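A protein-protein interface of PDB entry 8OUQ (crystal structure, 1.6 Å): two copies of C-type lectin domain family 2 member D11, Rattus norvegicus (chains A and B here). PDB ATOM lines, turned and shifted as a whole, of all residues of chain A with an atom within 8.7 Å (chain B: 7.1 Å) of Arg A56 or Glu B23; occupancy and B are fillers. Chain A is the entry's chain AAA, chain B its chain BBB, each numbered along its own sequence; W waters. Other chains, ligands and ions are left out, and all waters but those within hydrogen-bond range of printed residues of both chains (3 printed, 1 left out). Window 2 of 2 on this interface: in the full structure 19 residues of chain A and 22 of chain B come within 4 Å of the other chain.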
ATOM      1  N   PHE A  21       1.643 -29.824  12.867  1.00  0.00           N
ATOM      2  CA  PHE A  21       2.163 -31.202  12.883  1.00  0.00           C
ATOM      3  C   PHE A  21       1.024 -32.178  12.806  1.00  0.00           C
ATOM      4  O   PHE A  21       0.068 -32.068  13.587  1.00  0.00           O
ATOM      5  CB  PHE A  21       2.945 -31.473  14.183  1.00  0.00           C
ATOM      6  CG  PHE A  21       4.154 -30.615  14.315  1.00  0.00           C
ATOM      7  CD1 PHE A  21       4.052 -29.307  14.759  1.00  0.00           C
ATOM      8  CD2 PHE A  21       5.385 -31.109  13.901  1.00  0.00           C
ATOM      9  CE1 PHE A  21       5.191 -28.515  14.761  1.00  0.00           C
ATOM     10  CE2 PHE A  21       6.525 -30.321  13.983  1.00  0.00           C
ATOM     11  CZ  PHE A  21       6.409 -29.025  14.404  1.00  0.00           C
ATOM     12  N   GLU A  49      17.164 -21.889  15.121  1.00  0.00           N
ATOM     13  CA  GLU A  49      16.071 -21.839  16.130  1.00  0.00           C
ATOM     14  C   GLU A  49      14.916 -22.678  15.567  1.00  0.00           C
ATOM     15  O   GLU A  49      14.368 -23.527  16.299  1.00  0.00           O
ATOM     16  CB  GLU A  49      15.624 -20.395  16.442  1.00  0.00           C
ATOM     17  CG  GLU A  49      14.422 -20.205  17.409  1.00  0.00           C
ATOM     18  CD  GLU A  49      13.895 -18.774  17.683  1.00  0.00           C
ATOM     19  OE1 GLU A  49      14.016 -17.839  16.806  1.00  0.00           O
ATOM     20  OE2 GLU A  49      13.340 -18.554  18.790  1.00  0.00           O
ATOM     21  N   GLU A  50      14.527 -22.416  14.332  1.00  0.00           N
ATOM     22  CA  GLU A  50      13.404 -23.157  13.688  1.00  0.00           C
ATOM     23  C   GLU A  50      13.722 -24.659  13.534  1.00  0.00           C
ATOM     24  O   GLU A  50      12.897 -25.505  13.913  1.00  0.00           O
ATOM     25  CB  GLU A  50      13.094 -22.567  12.324  1.00  0.00           C
ATOM     26  CG  GLU A  50      12.493 -21.176  12.380  1.00  0.00           C
ATOM     27  CD  GLU A  50      12.353 -20.449  11.045  1.00  0.00           C
ATOM     28  OE1 GLU A  50      12.438 -21.072   9.962  1.00  0.00           O
ATOM     29  OE2 GLU A  50      12.152 -19.250  11.107  1.00  0.00           O
ATOM     30  N   LEU A  51      14.900 -24.983  13.026  1.00  0.00           N
ATOM     31  CA  LEU A  51      15.270 -26.411  12.875  1.00  0.00           C
ATOM     32  C   LEU A  51      15.337 -27.069  14.250  1.00  0.00           C
ATOM     33  O   LEU A  51      14.882 -28.215  14.367  1.00  0.00           O
ATOM     34  CB  LEU A  51      16.575 -26.548  12.100  1.00  0.00           C
ATOM     35  CG  LEU A  51      17.114 -27.969  11.912  1.00  0.00           C
ATOM     36  CD1 LEU A  51      16.064 -28.911  11.301  1.00  0.00           C
ATOM     37  CD2 LEU A  51      18.345 -27.964  11.039  1.00  0.00           C
ATOM     38  N   ASN A  52      15.877 -26.412  15.277  1.00  0.00           N
ATOM     39  CA  ASN A  52      15.983 -27.054  16.615  1.00  0.00           C
ATOM     40  C   ASN A  52      14.575 -27.317  17.134  1.00  0.00           C
ATOM     41  O   ASN A  52      14.346 -28.376  17.746  1.00  0.00           O
ATOM     42  CB  ASN A  52      16.743 -26.209  17.647  1.00  0.00           C
ATOM     43  CG  ASN A  52      18.236 -26.141  17.369  1.00  0.00           C
ATOM     44  OD1 ASN A  52      18.724 -26.863  16.521  1.00  0.00           O
ATOM     45  ND2 ASN A  52      18.894 -25.139  17.901  1.00  0.00           N
ATOM     46  N   PHE A  53      13.620 -26.426  16.871  1.00  0.00           N
ATOM     47  CA  PHE A  53      12.215 -26.596  17.326  1.00  0.00           C
ATOM     48  C   PHE A  53      11.597 -27.849  16.645  1.00  0.00           C
ATOM     49  O   PHE A  53      11.025 -28.669  17.343  1.00  0.00           O
ATOM     50  CB  PHE A  53      11.382 -25.332  17.079  1.00  0.00           C
ATOM     51  CG  PHE A  53       9.920 -25.611  17.256  1.00  0.00           C
ATOM     52  CD1 PHE A  53       9.347 -25.784  18.503  1.00  0.00           C
ATOM     53  CD2 PHE A  53       9.149 -25.785  16.115  1.00  0.00           C
ATOM     54  CE1 PHE A  53       8.003 -26.080  18.609  1.00  0.00           C
ATOM     55  CE2 PHE A  53       7.828 -26.127  16.245  1.00  0.00           C
ATOM     56  CZ  PHE A  53       7.254 -26.263  17.478  1.00  0.00           C
ATOM     57  N   LEU A  54      11.698 -27.975  15.328  1.00  0.00           N
ATOM     58  CA  LEU A  54      11.223 -29.167  14.550  1.00  0.00           C
ATOM     59  C   LEU A  54      11.852 -30.441  15.115  1.00  0.00           C
ATOM     60  O   LEU A  54      11.112 -31.401  15.362  1.00  0.00           O
ATOM     61  CB  LEU A  54      11.609 -28.976  13.071  1.00  0.00           C
ATOM     62  CG  LEU A  54      10.831 -27.877  12.396  1.00  0.00           C
ATOM     63  CD1 LEU A  54      11.232 -27.783  10.967  1.00  0.00           C
ATOM     64  CD2 LEU A  54       9.314 -28.015  12.596  1.00  0.00           C
ATOM     65  N   SER A  55      13.165 -30.416  15.340  1.00  0.00           N
ATOM     66  CA  SER A  55      13.953 -31.603  15.782  1.00  0.00           C
ATOM     67  C   SER A  55      13.615 -31.994  17.214  1.00  0.00           C
ATOM     68  O   SER A  55      13.820 -33.174  17.552  1.00  0.00           O
ATOM     69  CB  SER A  55      15.423 -31.389  15.642  1.00  0.00           C
ATOM     70  OG  SER A  55      15.722 -31.097  14.282  1.00  0.00           O
ATOM     71  N   ARG A  56      13.082 -31.099  18.034  1.00  0.00           N
ATOM     72  CA  ARG A  56      12.634 -31.417  19.386  1.00  0.00           C
ATOM     73  C   ARG A  56      11.176 -31.816  19.402  1.00  0.00           C
ATOM     74  O   ARG A  56      10.822 -32.810  20.029  1.00  0.00           O
ATOM     75  CB  ARG A  56      12.871 -30.191  20.281  1.00  0.00           C
ATOM     76  CG  ARG A  56      12.394 -30.371  21.711  1.00  0.00           C
ATOM     77  CD  ARG A  56      13.116 -29.351  22.595  1.00  0.00           C
ATOM     78  NE  ARG A  56      12.572 -29.385  23.941  1.00  0.00           N
ATOM     79  CZ  ARG A  56      13.048 -28.724  24.992  1.00  0.00           C
ATOM     80  NH1 ARG A  56      12.424 -28.796  26.157  1.00  0.00           N
ATOM     81  NH2 ARG A  56      14.114 -27.971  24.881  1.00  0.00           N
ATOM     82  N   TYR A  57      10.301 -31.071  18.722  1.00  0.00           N
ATOM     83  CA  TYR A  57       8.837 -31.284  18.843  1.00  0.00           C
ATOM     84  C   TYR A  57       8.455 -32.616  18.143  1.00  0.00           C
ATOM     85  O   TYR A  57       7.487 -33.243  18.562  1.00  0.00           O
ATOM     86  CB  TYR A  57       8.079 -30.020  18.368  1.00  0.00           C
ATOM     87  CG  TYR A  57       6.615 -30.017  18.726  1.00  0.00           C
ATOM     88  CD1 TYR A  57       6.196 -29.767  20.014  1.00  0.00           C
ATOM     89  CD2 TYR A  57       5.644 -30.303  17.792  1.00  0.00           C
ATOM     90  CE1 TYR A  57       4.866 -29.723  20.357  1.00  0.00           C
ATOM     91  CE2 TYR A  57       4.293 -30.339  18.130  1.00  0.00           C
ATOM     92  CZ  TYR A  57       3.901 -30.000  19.413  1.00  0.00           C
ATOM     93  OH  TYR A  57       2.561 -29.983  19.783  1.00  0.00           O
ATOM     94  N   LYS A  58       9.253 -33.067  17.158  1.00  0.00           N
ATOM     95  CA  LYS A  58       8.990 -34.328  16.415  1.00  0.00           C
ATOM     96  C   LYS A  58       9.067 -35.519  17.380  1.00  0.00           C
ATOM     97  O   LYS A  58       8.462 -36.562  17.060  1.00  0.00           O
ATOM     98  CB  LYS A  58       9.982 -34.553  15.278  1.00  0.00           C
ATOM     99  CG  LYS A  58      11.436 -34.715  15.670  1.00  0.00           C
ATOM    100  CD  LYS A  58      12.382 -34.968  14.488  1.00  0.00           C
ATOM    101  CE  LYS A  58      12.266 -36.360  13.929  1.00  0.00           C
ATOM    102  NZ  LYS A  58      12.589 -37.379  14.948  1.00  0.00           N
ATOM    103  N   GLY A  59       9.788 -35.401  18.493  1.00  0.00           N
ATOM    104  CA  GLY A  59       9.995 -36.573  19.379  1.00  0.00           C
ATOM    105  C   GLY A  59      10.633 -37.727  18.635  1.00  0.00           C
ATOM    106  O   GLY A  59      11.561 -37.482  17.803  1.00  0.00           O
ATOM    107  N   SER A  60      10.152 -38.943  18.880  1.00  0.00           N
ATOM    108  CA  SER A  60      10.777 -40.176  18.350  1.00  0.00           C
ATOM    109  C   SER A  60      10.188 -40.564  16.993  1.00  0.00           C
ATOM    110  O   SER A  60      10.460 -41.695  16.560  1.00  0.00           O
ATOM    111  CB  SER A  60      10.650 -41.291  19.348  1.00  0.00           C
ATOM    112  OG  SER A  60      11.449 -40.994  20.473  1.00  0.00           O
ATOM    113  N   PHE A  61       9.454 -39.674  16.320  1.00  0.00           N
ATOM    114  CA  PHE A  61       8.806 -40.018  15.033  1.00  0.00           C
ATOM    115  C   PHE A  61       9.404 -39.233  13.868  1.00  0.00           C
ATOM    116  O   PHE A  61       9.760 -38.082  13.976  1.00  0.00           O
ATOM    117  CB  PHE A  61       7.301 -39.960  15.162  1.00  0.00           C
ATOM    118  CG  PHE A  61       6.834 -40.801  16.319  1.00  0.00           C
ATOM    119  CD1 PHE A  61       7.178 -42.144  16.377  1.00  0.00           C
ATOM    120  CD2 PHE A  61       6.239 -40.221  17.429  1.00  0.00           C
ATOM    121  CE1 PHE A  61       6.788 -42.928  17.454  1.00  0.00           C
ATOM    122  CE2 PHE A  61       5.853 -41.004  18.510  1.00  0.00           C
ATOM    123  CZ  PHE A  61       6.119 -42.359  18.517  1.00  0.00           C
ATOM    124  N   TYR A  63       9.304 -37.157  10.450  1.00  0.00           N
ATOM    125  CA  TYR A  63       8.419 -36.134   9.845  1.00  0.00           C
ATOM    126  C   TYR A  63       8.874 -35.669   8.473  1.00  0.00           C
ATOM    127  O   TYR A  63      10.014 -35.224   8.279  1.00  0.00           O
ATOM    128  CB  TYR A  63       8.262 -34.903  10.734  1.00  0.00           C
ATOM    129  CG  TYR A  63       7.228 -35.072  11.818  1.00  0.00           C
ATOM    130  CD1 TYR A  63       7.529 -35.770  12.962  1.00  0.00           C
ATOM    131  CD2 TYR A  63       5.960 -34.554  11.673  1.00  0.00           C
ATOM    132  CE1 TYR A  63       6.592 -35.949  13.953  1.00  0.00           C
ATOM    133  CE2 TYR A  63       5.022 -34.667  12.673  1.00  0.00           C
ATOM    134  CZ  TYR A  63       5.339 -35.404  13.806  1.00  0.00           C
ATOM    135  OH  TYR A  63       4.419 -35.546  14.796  1.00  0.00           O
ATOM    136  N   LEU A  99      12.771 -35.551   8.528  1.00  0.00           N
ATOM    137  CA  LEU A  99      13.549 -35.501   9.786  1.00  0.00           C
ATOM    138  C   LEU A  99      13.506 -36.871  10.422  1.00  0.00           C
ATOM    139  O   LEU A  99      12.398 -37.381  10.630  1.00  0.00           O
ATOM    140  CB  LEU A  99      12.997 -34.438  10.721  1.00  0.00           C
ATOM    141  CG  LEU A  99      13.056 -33.037  10.162  1.00  0.00           C
ATOM    142  CD1 LEU A  99      12.514 -32.051  11.194  1.00  0.00           C
ATOM    143  CD2 LEU A  99      14.471 -32.758   9.740  1.00  0.00           C
ATOM    144  N   ASN A 100      14.678 -37.424  10.715  1.00  0.00           N
ATOM    145  CA  ASN A 100      14.747 -38.758  11.327  1.00  0.00           C
ATOM    146  C   ASN A 100      15.321 -38.631  12.714  1.00  0.00           C
ATOM    147  O   ASN A 100      15.318 -37.591  13.216  1.00  0.00           O
ATOM    148  CB  ASN A 100      15.429 -39.734  10.392  1.00  0.00           C
ATOM    149  CG  ASN A 100      16.929 -39.661  10.325  1.00  0.00           C
ATOM    150  OD1 ASN A 100      17.574 -38.731  10.806  1.00  0.00           O
ATOM    151  ND2 ASN A 100      17.452 -40.699   9.707  1.00  0.00           N
ATOM    152  N   ILE B  12       8.040 -19.523  22.488  1.00  0.00           N
ATOM    153  CA  ILE B  12       7.203 -20.346  21.560  1.00  0.00           C
ATOM    154  C   ILE B  12       5.745 -19.930  21.740  1.00  0.00           C
ATOM    155  O   ILE B  12       5.282 -19.903  22.897  1.00  0.00           O
ATOM    156  CB  ILE B  12       7.451 -21.844  21.807  1.00  0.00           C
ATOM    157  CG1 ILE B  12       8.917 -22.215  21.572  1.00  0.00           C
ATOM    158  CG2 ILE B  12       6.597 -22.703  20.900  1.00  0.00           C
ATOM    159  CD1 ILE B  12       9.281 -23.544  22.184  1.00  0.00           C
ATOM    160  N   TYR B  20       8.543 -20.188  27.454  1.00  0.00           N
ATOM    161  CA  TYR B  20      10.020 -20.273  27.533  1.00  0.00           C
ATOM    162  C   TYR B  20      10.383 -21.575  28.265  1.00  0.00           C
ATOM    163  O   TYR B  20       9.710 -21.931  29.253  1.00  0.00           O
ATOM    164  CB  TYR B  20      10.615 -19.093  28.304  1.00  0.00           C
ATOM    165  CG  TYR B  20      12.112 -19.046  28.265  1.00  0.00           C
ATOM    166  CD1 TYR B  20      12.745 -18.655  27.091  1.00  0.00           C
ATOM    167  CD2 TYR B  20      12.884 -19.363  29.338  1.00  0.00           C
ATOM    168  CE1 TYR B  20      14.118 -18.593  26.991  1.00  0.00           C
ATOM    169  CE2 TYR B  20      14.262 -19.336  29.256  1.00  0.00           C
ATOM    170  CZ  TYR B  20      14.882 -18.930  28.090  1.00  0.00           C
ATOM    171  OH  TYR B  20      16.235 -18.842  27.924  1.00  0.00           O
ATOM    172  N   PHE B  21      11.448 -22.211  27.815  1.00  0.00           N
ATOM    173  CA  PHE B  21      11.928 -23.446  28.469  1.00  0.00           C
ATOM    174  C   PHE B  21      13.413 -23.330  28.793  1.00  0.00           C
ATOM    175  O   PHE B  21      14.244 -23.035  27.900  1.00  0.00           O
ATOM    176  CB  PHE B  21      11.699 -24.642  27.538  1.00  0.00           C
ATOM    177  CG  PHE B  21      10.255 -24.908  27.242  1.00  0.00           C
ATOM    178  CD1 PHE B  21       9.590 -24.181  26.281  1.00  0.00           C
ATOM    179  CD2 PHE B  21       9.549 -25.852  27.975  1.00  0.00           C
ATOM    180  CE1 PHE B  21       8.228 -24.393  26.075  1.00  0.00           C
ATOM    181  CE2 PHE B  21       8.199 -26.099  27.745  1.00  0.00           C
ATOM    182  CZ  PHE B  21       7.550 -25.368  26.767  1.00  0.00           C
ATOM    183  N   SER B  22      13.770 -23.596  30.049  1.00  0.00           N
ATOM    184  CA  SER B  22      15.199 -23.632  30.408  1.00  0.00           C
ATOM    185  C   SER B  22      15.803 -24.956  29.963  1.00  0.00           C
ATOM    186  O   SER B  22      15.068 -25.945  29.792  1.00  0.00           O
ATOM    187  CB  SER B  22      15.412 -23.428  31.933  1.00  0.00           C
ATOM    188  OG  SER B  22      15.326 -24.674  32.648  1.00  0.00           O
ATOM    189  N   GLU B  23      17.113 -24.986  29.823  1.00  0.00           N
ATOM    190  CA  GLU B  23      17.824 -26.283  29.710  1.00  0.00           C
ATOM    191  C   GLU B  23      18.773 -26.452  30.896  1.00  0.00           C
ATOM    192  O   GLU B  23      19.841 -27.079  30.753  1.00  0.00           O
ATOM    193  CB  GLU B  23      18.585 -26.312  28.383  1.00  0.00           C
ATOM    194  CG  GLU B  23      17.705 -26.406  27.146  1.00  0.00           C
ATOM    195  CD  GLU B  23      18.379 -27.166  25.990  1.00  0.00           C
ATOM    196  OE1 GLU B  23      19.587 -26.959  25.773  1.00  0.00           O
ATOM    197  OE2 GLU B  23      17.738 -28.058  25.380  1.00  0.00           O
ATOM    198  N   TYR B  24      18.417 -25.873  32.031  1.00  0.00           N
ATOM    199  CA  TYR B  24      19.282 -25.836  33.232  1.00  0.00           C
ATOM    200  C   TYR B  24      18.354 -26.150  34.402  1.00  0.00           C
ATOM    201  O   TYR B  24      17.241 -25.583  34.423  1.00  0.00           O
ATOM    202  CB  TYR B  24      19.980 -24.476  33.270  1.00  0.00           C
ATOM    203  CG  TYR B  24      21.085 -24.359  34.291  1.00  0.00           C
ATOM    204  CD1 TYR B  24      20.766 -24.320  35.629  1.00  0.00           C
ATOM    205  CD2 TYR B  24      22.394 -24.118  33.902  1.00  0.00           C
ATOM    206  CE1 TYR B  24      21.759 -24.245  36.602  1.00  0.00           C
ATOM    207  CE2 TYR B  24      23.382 -23.952  34.861  1.00  0.00           C
ATOM    208  CZ  TYR B  24      23.057 -24.007  36.205  1.00  0.00           C
ATOM    209  OH  TYR B  24      24.067 -23.878  37.115  1.00  0.00           O
ATOM    210  N   ALA B  25      18.743 -27.067  35.280  1.00  0.00           N
ATOM    211  CA  ALA B  25      17.867 -27.454  36.415  1.00  0.00           C
ATOM    212  C   ALA B  25      18.199 -26.593  37.636  1.00  0.00           C
ATOM    213  O   ALA B  25      19.406 -26.428  37.981  1.00  0.00           O
ATOM    214  CB  ALA B  25      17.971 -28.915  36.709  1.00  0.00           C
ATOM    215  N   ARG B  56       4.381 -32.308  25.598  1.00  0.00           N
ATOM    216  CA  ARG B  56       5.123 -32.860  24.465  1.00  0.00           C
ATOM    217  C   ARG B  56       6.503 -32.213  24.385  1.00  0.00           C
ATOM    218  O   ARG B  56       7.481 -32.908  24.155  1.00  0.00           O
ATOM    219  CB  ARG B  56       4.343 -32.582  23.183  1.00  0.00           C
ATOM    220  CG  ARG B  56       5.048 -33.072  21.936  1.00  0.00           C
ATOM    221  CD  ARG B  56       4.044 -33.204  20.816  1.00  0.00           C
ATOM    222  NE  ARG B  56       4.704 -33.507  19.567  1.00  0.00           N
ATOM    223  CZ  ARG B  56       4.081 -33.845  18.464  1.00  0.00           C
ATOM    224  NH1 ARG B  56       4.781 -34.062  17.363  1.00  0.00           N
ATOM    225  NH2 ARG B  56       2.771 -33.842  18.418  1.00  0.00           N
ATOM    226  N   TYR B  57       6.558 -30.883  24.449  1.00  0.00           N
ATOM    227  CA  TYR B  57       7.833 -30.169  24.254  1.00  0.00           C
ATOM    228  C   TYR B  57       8.825 -30.475  25.396  1.00  0.00           C
ATOM    229  O   TYR B  57      10.034 -30.399  25.113  1.00  0.00           O
ATOM    230  CB  TYR B  57       7.580 -28.672  24.006  1.00  0.00           C
ATOM    231  CG  TYR B  57       8.772 -27.959  23.441  1.00  0.00           C
ATOM    232  CD1 TYR B  57       9.173 -28.068  22.124  1.00  0.00           C
ATOM    233  CD2 TYR B  57       9.539 -27.168  24.289  1.00  0.00           C
ATOM    234  CE1 TYR B  57      10.255 -27.361  21.641  1.00  0.00           C
ATOM    235  CE2 TYR B  57      10.666 -26.504  23.832  1.00  0.00           C
ATOM    236  CZ  TYR B  57      10.980 -26.546  22.490  1.00  0.00           C
ATOM    237  OH  TYR B  57      12.104 -25.871  22.040  1.00  0.00           O
ATOM    238  N   LYS B  58       8.348 -30.852  26.581  1.00  0.00           N
ATOM    239  CA  LYS B  58       9.270 -31.110  27.724  1.00  0.00           C
ATOM    240  C   LYS B  58      10.209 -32.312  27.438  1.00  0.00           C
ATOM    241  O   LYS B  58      11.246 -32.428  28.134  1.00  0.00           O
ATOM    242  CB  LYS B  58       8.468 -31.421  28.992  1.00  0.00           C
ATOM    243  CG  LYS B  58       7.520 -32.596  28.899  1.00  0.00           C
ATOM    244  CD  LYS B  58       6.750 -32.931  30.182  1.00  0.00           C
ATOM    245  CE  LYS B  58       7.597 -33.417  31.325  1.00  0.00           C
ATOM    246  NZ  LYS B  58       8.236 -34.707  30.966  1.00  0.00           N
ATOM    247  N   GLY B  59       9.819 -33.225  26.547  1.00  0.00           N
ATOM    248  CA  GLY B  59      10.544 -34.497  26.349  1.00  0.00           C
ATOM    249  C   GLY B  59      10.602 -35.348  27.617  1.00  0.00           C
ATOM    250  O   GLY B  59       9.593 -35.397  28.418  1.00  0.00           O
ATOM    251  N   PHE B  61      12.349 -34.844  30.357  1.00  0.00           N
ATOM    252  CA  PHE B  61      12.825 -34.093  31.548  1.00  0.00           C
ATOM    253  C   PHE B  61      11.633 -33.542  32.337  1.00  0.00           C
ATOM    254  O   PHE B  61      10.673 -33.119  31.725  1.00  0.00           O
ATOM    255  CB  PHE B  61      13.744 -32.963  31.087  1.00  0.00           C
ATOM    256  CG  PHE B  61      15.025 -33.455  30.469  1.00  0.00           C
ATOM    257  CD1 PHE B  61      16.134 -33.714  31.257  1.00  0.00           C
ATOM    258  CD2 PHE B  61      15.103 -33.705  29.106  1.00  0.00           C
ATOM    259  CE1 PHE B  61      17.312 -34.177  30.684  1.00  0.00           C
ATOM    260  CE2 PHE B  61      16.279 -34.169  28.535  1.00  0.00           C
ATOM    261  CZ  PHE B  61      17.374 -34.420  29.329  1.00  0.00           C
ATOM    262  N   TYR B  63       9.706 -30.668  34.353  1.00  0.00           N
ATOM    263  CA  TYR B  63       9.648 -29.189  34.274  1.00  0.00           C
ATOM    264  C   TYR B  63       8.792 -28.643  35.392  1.00  0.00           C
ATOM    265  O   TYR B  63       7.588 -28.942  35.516  1.00  0.00           O
ATOM    266  CB  TYR B  63       9.187 -28.659  32.904  1.00  0.00           C
ATOM    267  CG  TYR B  63      10.279 -28.610  31.868  1.00  0.00           C
ATOM    268  CD1 TYR B  63      10.769 -29.751  31.243  1.00  0.00           C
ATOM    269  CD2 TYR B  63      10.869 -27.407  31.558  1.00  0.00           C
ATOM    270  CE1 TYR B  63      11.804 -29.676  30.320  1.00  0.00           C
ATOM    271  CE2 TYR B  63      11.870 -27.313  30.621  1.00  0.00           C
ATOM    272  CZ  TYR B  63      12.360 -28.452  30.015  1.00  0.00           C
ATOM    273  OH  TYR B  63      13.370 -28.255  29.123  1.00  0.00           O
ATOM    274  N   ARG B 114      14.496 -28.522  35.452  1.00  0.00           N
ATOM    275  CA  ARG B 114      14.277 -27.496  34.406  1.00  0.00           C
ATOM    276  C   ARG B 114      12.945 -26.799  34.709  1.00  0.00           C
ATOM    277  O   ARG B 114      12.100 -27.322  35.460  1.00  0.00           O
ATOM    278  CB  ARG B 114      14.273 -28.118  33.024  1.00  0.00           C
ATOM    279  CG  ARG B 114      15.631 -28.685  32.667  1.00  0.00           C
ATOM    280  CD  ARG B 114      15.499 -29.408  31.365  1.00  0.00           C
ATOM    281  NE  ARG B 114      16.744 -29.968  30.911  1.00  0.00           N
ATOM    282  CZ  ARG B 114      17.048 -30.178  29.622  1.00  0.00           C
ATOM    283  NH1 ARG B 114      18.204 -30.738  29.316  1.00  0.00           N
ATOM    284  NH2 ARG B 114      16.205 -29.836  28.650  1.00  0.00           N
ATOM    285  N   TRP B 115      12.757 -25.604  34.163  1.00  0.00           N
ATOM    286  CA  TRP B 115      11.506 -24.862  34.376  1.00  0.00           C
ATOM    287  C   TRP B 115      11.020 -24.308  33.053  1.00  0.00           C
ATOM    288  O   TRP B 115      11.810 -24.164  32.084  1.00  0.00           O
ATOM    289  CB  TRP B 115      11.652 -23.806  35.453  1.00  0.00           C
ATOM    290  CG  TRP B 115      12.506 -22.620  35.085  1.00  0.00           C
ATOM    291  CD1 TRP B 115      12.080 -21.453  34.522  1.00  0.00           C
ATOM    292  CD2 TRP B 115      13.914 -22.509  35.210  1.00  0.00           C
ATOM    293  NE1 TRP B 115      13.166 -20.673  34.240  1.00  0.00           N
ATOM    294  CE2 TRP B 115      14.305 -21.275  34.669  1.00  0.00           C
ATOM    295  CE3 TRP B 115      14.903 -23.395  35.671  1.00  0.00           C
ATOM    296  CZ2 TRP B 115      15.640 -20.832  34.695  1.00  0.00           C
ATOM    297  CZ3 TRP B 115      16.202 -22.930  35.761  1.00  0.00           C
ATOM    298  CH2 TRP B 115      16.566 -21.672  35.242  1.00  0.00           C
HETATM  299  O   HOH W   1       8.561 -34.530  21.833  1.00  0.00           O
HETATM  300  O   HOH W   2      13.806 -25.959  20.173  1.00  0.00           O
HETATM  301  O   HOH W   3       1.833 -34.476  15.828  1.00  0.00           O
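OE2 of Glu B23 is in salt-bridge range of NH2 of Arg A56, 3.7 Å away. NE of Arg A56 lies within hydrogen-bond range of O of Tyr B57 (3.0 Å). NH1 of Arg A56 lies within hydrogen-bond range of OH of Tyr B63 (3.2 Å). The guanidinium group (NE) of Arg B56 lies within hydrogen-bond range of the backbone carbonyl oxygen (O) of Tyr A57, at 3.0 Å. The side-chain hydroxyl (OH) of Tyr A63 is in hydrogen-bond range of the guanidinium group (NH1) of Arg B56 (3.0 Å).
The backbone carbonyl oxygen of Tyr A63 is in hydrogen-bond range of the backbone NH of Leu A99 (2.8 Å). The backbone carbonyl oxygen (O) of Ser B22 lies within hydrogen-bond range of the side-chain hydroxyl (OH) of Tyr B63, at 2.9 Å. The side-chain hydroxyl of Tyr B63 is in hydrogen-bond range of the guanidinium group of Arg B114, at 3.3 Å.
Among the printed residues, pairs that only touch across the chains: Phe A53 with Tyr B57 (3.6 Å).
Of the printed residues of chain B, Arg A56 touches Glu B23, Tyr B57 and Tyr B63. Glu B23 touches one residue of chain A. Of the printed residues of chain B, Tyr A57 touches Arg B56 (3.0 Å). Printed residues of chain A within 4 Å of Tyr B57: Phe A53 (3.6 Å) and Arg A56 (3.0 Å). Printed residues of chain B within 4 Å of Phe A53: Tyr B57 (3.6 Å). Printed residues of chain A within 4 Å of Tyr B63: Arg A56. Of the printed residues of chain A, Arg B56 touches Tyr A57 and Tyr A63. The nearest residue of chain A that does not touch Glu B23 is Asn A52 (8.0 Å).
Of the 17 printed residues of chain A, 4 touch a printed residue of chain B. Hydrophobic or aromatic side chains of chain B that line the printed part of chain A: Tyr B57 and Tyr B63.
Arg A56 touches Tyr B57, and with the chains exchanged Tyr A57 touches Arg B56. Arg A56 touches Tyr B63, and with the chains exchanged Tyr A63 touches Arg B56. 7 positions are printed for both chains. Of the 6 pairs that touch across the chains among the printed residues, 4 have their exchanged pair printed and touching as well.
Water W2 lies within hydrogen-bond range of the side-chain hydroxyl of Tyr B57, the backbone NH of Phe A53 and the backbone carbonyl oxygen of Asn A52. Water W3 lies within hydrogen-bond range of NH2 of Arg B56 and OH of Tyr A63. Water W1 lies within hydrogen-bond range of the backbone carbonyl oxygen of Arg B56 (3.0 Å) and the backbone carbonyl oxygen of Arg A56 (3.4 Å).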
